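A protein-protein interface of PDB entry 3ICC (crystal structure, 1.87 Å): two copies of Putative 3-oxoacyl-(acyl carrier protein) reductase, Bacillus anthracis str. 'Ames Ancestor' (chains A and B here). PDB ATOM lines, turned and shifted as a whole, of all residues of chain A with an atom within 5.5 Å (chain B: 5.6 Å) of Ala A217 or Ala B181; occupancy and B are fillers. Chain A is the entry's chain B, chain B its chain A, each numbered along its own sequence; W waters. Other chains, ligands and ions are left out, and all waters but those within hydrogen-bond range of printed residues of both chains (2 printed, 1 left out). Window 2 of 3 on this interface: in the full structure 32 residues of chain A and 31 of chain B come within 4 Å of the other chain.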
ATOM      1  N   THR A 214      -7.705 -25.636  24.485  1.00  0.00           N
ATOM      2  CA  THR A 214      -8.234 -26.675  23.573  1.00  0.00           C
ATOM      3  C   THR A 214      -9.530 -27.345  24.041  1.00  0.00           C
ATOM      4  O   THR A 214     -10.199 -28.002  23.246  1.00  0.00           O
ATOM      5  CB  THR A 214      -7.233 -27.801  23.340  1.00  0.00           C
ATOM      6  OG1 THR A 214      -7.005 -28.483  24.580  1.00  0.00           O
ATOM      7  CG2 THR A 214      -5.952 -27.253  22.787  1.00  0.00           C
ATOM      8  N   ILE A 215      -9.869 -27.210  25.316  1.00  0.00           N
ATOM      9  CA  ILE A 215     -11.116 -27.795  25.809  1.00  0.00           C
ATOM     10  C   ILE A 215     -12.363 -27.085  25.263  1.00  0.00           C
ATOM     11  O   ILE A 215     -13.444 -27.664  25.257  1.00  0.00           O
ATOM     12  CB  ILE A 215     -11.194 -27.817  27.364  1.00  0.00           C
ATOM     13  CG1 ILE A 215     -11.156 -26.406  27.948  1.00  0.00           C
ATOM     14  CG2 ILE A 215     -10.095 -28.715  27.935  1.00  0.00           C
ATOM     15  CD1 ILE A 215     -11.370 -26.403  29.458  1.00  0.00           C
ATOM     16  N   SER A 216     -12.217 -25.825  24.860  1.00  0.00           N
ATOM     17  CA  SER A 216     -13.304 -25.061  24.239  1.00  0.00           C
ATOM     18  C   SER A 216     -13.584 -25.532  22.808  1.00  0.00           C
ATOM     19  O   SER A 216     -12.659 -25.774  22.056  1.00  0.00           O
ATOM     20  CB  SER A 216     -12.940 -23.571  24.169  1.00  0.00           C
ATOM     21  OG  SER A 216     -13.801 -22.903  23.272  1.00  0.00           O
ATOM     22  N   ALA A 217     -14.862 -25.624  22.421  1.00  0.00           N
ATOM     23  CA  ALA A 217     -15.197 -25.931  21.029  1.00  0.00           C
ATOM     24  C   ALA A 217     -14.598 -24.901  20.048  1.00  0.00           C
ATOM     25  O   ALA A 217     -14.427 -25.187  18.855  1.00  0.00           O
ATOM     26  CB  ALA A 217     -16.695 -25.996  20.855  1.00  0.00           C
ATOM     27  N   PHE A 218     -14.293 -23.701  20.551  1.00  0.00           N
ATOM     28  CA  PHE A 218     -13.731 -22.637  19.708  1.00  0.00           C
ATOM     29  C   PHE A 218     -12.227 -22.497  19.742  1.00  0.00           C
ATOM     30  O   PHE A 218     -11.703 -21.595  19.083  1.00  0.00           O
ATOM     31  CB  PHE A 218     -14.388 -21.299  20.066  1.00  0.00           C
ATOM     32  CG  PHE A 218     -15.867 -21.338  19.965  1.00  0.00           C
ATOM     33  CD1 PHE A 218     -16.481 -21.281  18.733  1.00  0.00           C
ATOM     34  CD2 PHE A 218     -16.654 -21.417  21.102  1.00  0.00           C
ATOM     35  CE1 PHE A 218     -17.881 -21.301  18.612  1.00  0.00           C
ATOM     36  CE2 PHE A 218     -18.034 -21.445  21.002  1.00  0.00           C
ATOM     37  CZ  PHE A 218     -18.650 -21.400  19.742  1.00  0.00           C
ATOM     38  N   ASN A 219     -11.544 -23.359  20.502  1.00  0.00           N
ATOM     39  CA  ASN A 219     -10.069 -23.367  20.587  1.00  0.00           C
ATOM     40  C   ASN A 219      -9.471 -21.997  20.952  1.00  0.00           C
ATOM     41  O   ASN A 219      -8.432 -21.585  20.403  1.00  0.00           O
ATOM     42  CB  ASN A 219      -9.438 -23.935  19.295  1.00  0.00           C
ATOM     43  CG  ASN A 219      -7.921 -24.243  19.451  1.00  0.00           C
ATOM     44  OD1 ASN A 219      -7.454 -24.618  20.533  1.00  0.00           O
ATOM     45  ND2 ASN A 219      -7.158 -24.092  18.355  1.00  0.00           N
ATOM     46  N   GLY A 251     -17.667 -21.302  26.092  1.00  0.00           N
ATOM     47  CA  GLY A 251     -17.293 -21.549  24.690  1.00  0.00           C
ATOM     48  C   GLY A 251     -17.346 -23.041  24.365  1.00  0.00           C
ATOM     49  O   GLY A 251     -16.400 -23.609  23.749  1.00  0.00           O
ATOM     50  N   GLY A 252     -18.420 -23.697  24.819  1.00  0.00           N
ATOM     51  CA  GLY A 252     -18.580 -25.152  24.632  1.00  0.00           C
ATOM     52  C   GLY A 252     -17.392 -25.964  25.125  1.00  0.00           C
ATOM     53  O   GLY A 252     -16.846 -26.821  24.386  1.00  0.00           O
ATOM     54  N   SER A 253     -16.956 -25.690  26.342  1.00  0.00           N
ATOM     55  CA  SER A 253     -15.824 -26.409  26.926  1.00  0.00           C
ATOM     56  C   SER A 253     -16.331 -27.788  27.316  1.00  0.00           C
ATOM     57  O   SER A 253     -17.394 -27.886  27.947  1.00  0.00           O
ATOM     58  CB  SER A 253     -15.245 -25.693  28.172  1.00  0.00           C
ATOM     59  OG  SER A 253     -14.592 -24.482  27.829  1.00  0.00           O
ATOM     60  N   LEU A 255     -17.775 -30.444  25.824  1.00  0.00           N
ATOM     61  CA  LEU A 255     -19.137 -30.866  25.442  1.00  0.00           C
ATOM     62  C   LEU A 255     -19.349 -32.423  25.433  1.00  0.00           C
ATOM     63  O   LEU A 255     -18.414 -33.173  25.096  1.00  0.00           O
ATOM     64  CB  LEU A 255     -19.478 -30.253  24.079  1.00  0.00           C
ATOM     65  CG  LEU A 255     -19.883 -28.786  24.158  1.00  0.00           C
ATOM     66  CD1 LEU A 255     -19.844 -28.134  22.771  1.00  0.00           C
ATOM     67  CD2 LEU A 255     -21.271 -28.647  24.779  1.00  0.00           C
ATOM     68  N   ALA B 176     -22.646 -28.790  18.259  1.00  0.00           N
ATOM     69  CA  ALA B 176     -21.952 -27.608  18.773  1.00  0.00           C
ATOM     70  C   ALA B 176     -20.463 -27.862  18.824  1.00  0.00           C
ATOM     71  O   ALA B 176     -19.640 -26.967  18.536  1.00  0.00           O
ATOM     72  CB  ALA B 176     -22.478 -27.251  20.157  1.00  0.00           C
ATOM     73  N   LYS B 177     -20.087 -29.077  19.188  1.00  0.00           N
ATOM     74  CA  LYS B 177     -18.660 -29.351  19.260  1.00  0.00           C
ATOM     75  C   LYS B 177     -18.033 -29.288  17.864  1.00  0.00           C
ATOM     76  O   LYS B 177     -16.956 -28.736  17.697  1.00  0.00           O
ATOM     77  CB  LYS B 177     -18.376 -30.710  19.885  1.00  0.00           C
ATOM     78  CG  LYS B 177     -16.918 -30.975  19.990  1.00  0.00           C
ATOM     79  CD  LYS B 177     -16.645 -32.211  20.793  1.00  0.00           C
ATOM     80  CE  LYS B 177     -15.147 -32.447  20.864  1.00  0.00           C
ATOM     81  NZ  LYS B 177     -14.904 -33.659  21.697  1.00  0.00           N
ATOM     82  N   GLN B 178     -18.708 -29.875  16.886  1.00  0.00           N
ATOM     83  CA  GLN B 178     -18.212 -29.908  15.538  1.00  0.00           C
ATOM     84  C   GLN B 178     -18.167 -28.501  14.944  1.00  0.00           C
ATOM     85  O   GLN B 178     -17.189 -28.123  14.298  1.00  0.00           O
ATOM     86  CB  GLN B 178     -19.056 -30.824  14.653  1.00  0.00           C
ATOM     87  CG  GLN B 178     -18.509 -31.003  13.227  1.00  0.00           C
ATOM     88  CD  GLN B 178     -19.454 -31.796  12.357  1.00  0.00           C
ATOM     89  OE1 GLN B 178     -20.319 -32.497  12.852  1.00  0.00           O
ATOM     90  NE2 GLN B 178     -19.298 -31.678  11.060  1.00  0.00           N
ATOM     91  N   LEU B 179     -19.225 -27.729  15.113  1.00  0.00           N
ATOM     92  CA  LEU B 179     -19.314 -26.468  14.377  1.00  0.00           C
ATOM     93  C   LEU B 179     -18.527 -25.279  14.978  1.00  0.00           C
ATOM     94  O   LEU B 179     -18.372 -24.224  14.325  1.00  0.00           O
ATOM     95  CB  LEU B 179     -20.755 -26.074  14.139  1.00  0.00           C
ATOM     96  CG  LEU B 179     -21.531 -27.156  13.366  1.00  0.00           C
ATOM     97  CD1 LEU B 179     -22.956 -26.694  13.119  1.00  0.00           C
ATOM     98  CD2 LEU B 179     -20.812 -27.503  12.056  1.00  0.00           C
ATOM     99  N   GLY B 180     -17.986 -25.462  16.176  1.00  0.00           N
ATOM    100  CA  GLY B 180     -17.236 -24.385  16.825  1.00  0.00           C
ATOM    101  C   GLY B 180     -16.002 -24.010  16.048  1.00  0.00           C
ATOM    102  O   GLY B 180     -15.513 -22.890  16.149  1.00  0.00           O
ATOM    103  N   ALA B 181     -15.497 -24.944  15.259  1.00  0.00           N
ATOM    104  CA  ALA B 181     -14.333 -24.680  14.419  1.00  0.00           C
ATOM    105  C   ALA B 181     -14.634 -23.544  13.441  1.00  0.00           C
ATOM    106  O   ALA B 181     -13.721 -22.841  13.019  1.00  0.00           O
ATOM    107  CB  ALA B 181     -13.933 -25.927  13.670  1.00  0.00           C
ATOM    108  N   ARG B 182     -15.911 -23.344  13.101  1.00  0.00           N
ATOM    109  CA  ARG B 182     -16.291 -22.247  12.210  1.00  0.00           C
ATOM    110  C   ARG B 182     -16.916 -21.050  12.951  1.00  0.00           C
ATOM    111  O   ARG B 182     -17.423 -20.127  12.318  1.00  0.00           O
ATOM    112  CB  ARG B 182     -17.271 -22.768  11.144  1.00  0.00           C
ATOM    113  CG  ARG B 182     -16.666 -23.818  10.193  1.00  0.00           C
ATOM    114  CD  ARG B 182     -17.729 -24.234   9.137  1.00  0.00           C
ATOM    115  NE  ARG B 182     -18.191 -23.040   8.457  1.00  0.00           N
ATOM    116  CZ  ARG B 182     -19.295 -22.924   7.726  1.00  0.00           C
ATOM    117  NH1 ARG B 182     -20.075 -23.962   7.470  1.00  0.00           N
ATOM    118  NH2 ARG B 182     -19.580 -21.737   7.215  1.00  0.00           N
ATOM    119  N   GLY B 183     -16.834 -21.051  14.277  1.00  0.00           N
ATOM    120  CA  GLY B 183     -17.414 -19.996  15.088  1.00  0.00           C
ATOM    121  C   GLY B 183     -18.919 -20.067  15.117  1.00  0.00           C
ATOM    122  O   GLY B 183     -19.606 -19.122  15.615  1.00  0.00           O
ATOM    123  N   ILE B 184     -19.479 -21.156  14.607  1.00  0.00           N
ATOM    124  CA  ILE B 184     -20.961 -21.287  14.565  1.00  0.00           C
ATOM    125  C   ILE B 184     -21.453 -21.856  15.889  1.00  0.00           C
ATOM    126  O   ILE B 184     -20.960 -22.897  16.326  1.00  0.00           O
ATOM    127  CB  ILE B 184     -21.438 -22.210  13.372  1.00  0.00           C
ATOM    128  CG1 ILE B 184     -21.107 -21.611  12.017  1.00  0.00           C
ATOM    129  CG2 ILE B 184     -23.016 -22.454  13.417  1.00  0.00           C
ATOM    130  CD1 ILE B 184     -21.364 -22.540  10.840  1.00  0.00           C
ATOM    131  N   THR B 243     -22.782 -22.007  23.559  1.00  0.00           N
ATOM    132  CA  THR B 243     -23.040 -23.036  22.563  1.00  0.00           C
ATOM    133  C   THR B 243     -23.272 -24.391  23.185  1.00  0.00           C
ATOM    134  O   THR B 243     -22.810 -24.658  24.292  1.00  0.00           O
ATOM    135  CB  THR B 243     -21.937 -23.133  21.502  1.00  0.00           C
ATOM    136  OG1 THR B 243     -22.424 -23.854  20.374  1.00  0.00           O
ATOM    137  CG2 THR B 243     -20.659 -23.802  22.067  1.00  0.00           C
HETATM  138  O   HOH W   1     -16.707 -34.880  23.256  1.00  0.00           O
HETATM  139  O   HOH W   2     -14.749 -27.327  17.307  1.00  0.00           O
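OG of Ser A216 sits at hydrogen-bond distance from N of Phe A218. The backbone NH (N) of Ala A217 lies within hydrogen-bond range of the backbone carbonyl oxygen (O) of Gly A251 (2.9 Å). N of Ala A217 lies within hydrogen-bond range of O of Gly A252 (3.0 Å).
Among the printed residues, pairs that only touch across the chains: Phe A218 with Gly B180 (3.2 Å), Ala A217 with Gly B180 (3.4 Å), Gly A252 with Thr B243 (3.5 Å), Phe A218 with Thr B243 (3.7 Å), Leu A255 with Lys B177 (3.7 Å), Ala A217 with Ala B181 (3.8 Å), Phe A218 with Gly B183 (3.8 Å), Leu A255 with Ala B176 (3.8 Å) and Ala A217 with Ala B176 (3.9 Å).
Ala A217 touches just these residues of chain B: Ala B176 (3.9 Å), Gly B180 (3.4 Å) and Ala B181 (3.8 Å). Printed residues of chain B within 4 Å of Gly A252: Thr B243 (3.5 Å). Of the printed residues of chain B, Leu A255 touches Ala B176 (3.8 Å) and Lys B177 (3.7 Å). Printed residues of chain A within 4 Å of Gly B180: Ala A217 and Phe A218. Of chain A, only Ala A217 comes within 4 Å of Ala B181. Of the printed residues of chain A, Thr B243 touches Phe A218 and Gly A252. The nearest residue of chain B that does not touch Ala A217 is Lys B177 (4.2 Å). The nearest residue of chain A that does not touch Ala B181 is Phe A218 (5.1 Å). The nearest printed residue of chain A that does not touch Thr B243 is Gly A251 (4.1 Å).
Hydrophobic or aromatic side chains of chain B that line the printed part of chain A: Ala B176. Along chain B the printed residues that touch a printed residue of chain A span positions 176 to 243. Of the 10 printed residues of chain A, 4 touch a printed residue of chain B. Printed residues of chain A that touch a printed residue of chain B: Ala A217, Phe A218, Gly A252 and Leu A255. Hydrophobic or aromatic side chains of chain A that line the printed part of chain B: Ala A217, Phe A218 and Leu A255. Among the printed residues, no Asp or Glu carboxylate lies within 4 Å of a Lys or Arg side-chain nitrogen of the other chain.
No position is printed for both chains.
Water W2 lies within hydrogen-bond range of the backbone carbonyl oxygen of Lys B177 (2.6 Å), the backbone carbonyl oxygen of Ala A217 (2.7 Å) and the backbone NH of Ala B181 (3.2 Å). Water W1 lies within hydrogen-bond range of the side-chain amino group of Lys B177 (2.7 Å) and the backbone carbonyl oxygen of Leu A255 (3.0 Å).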
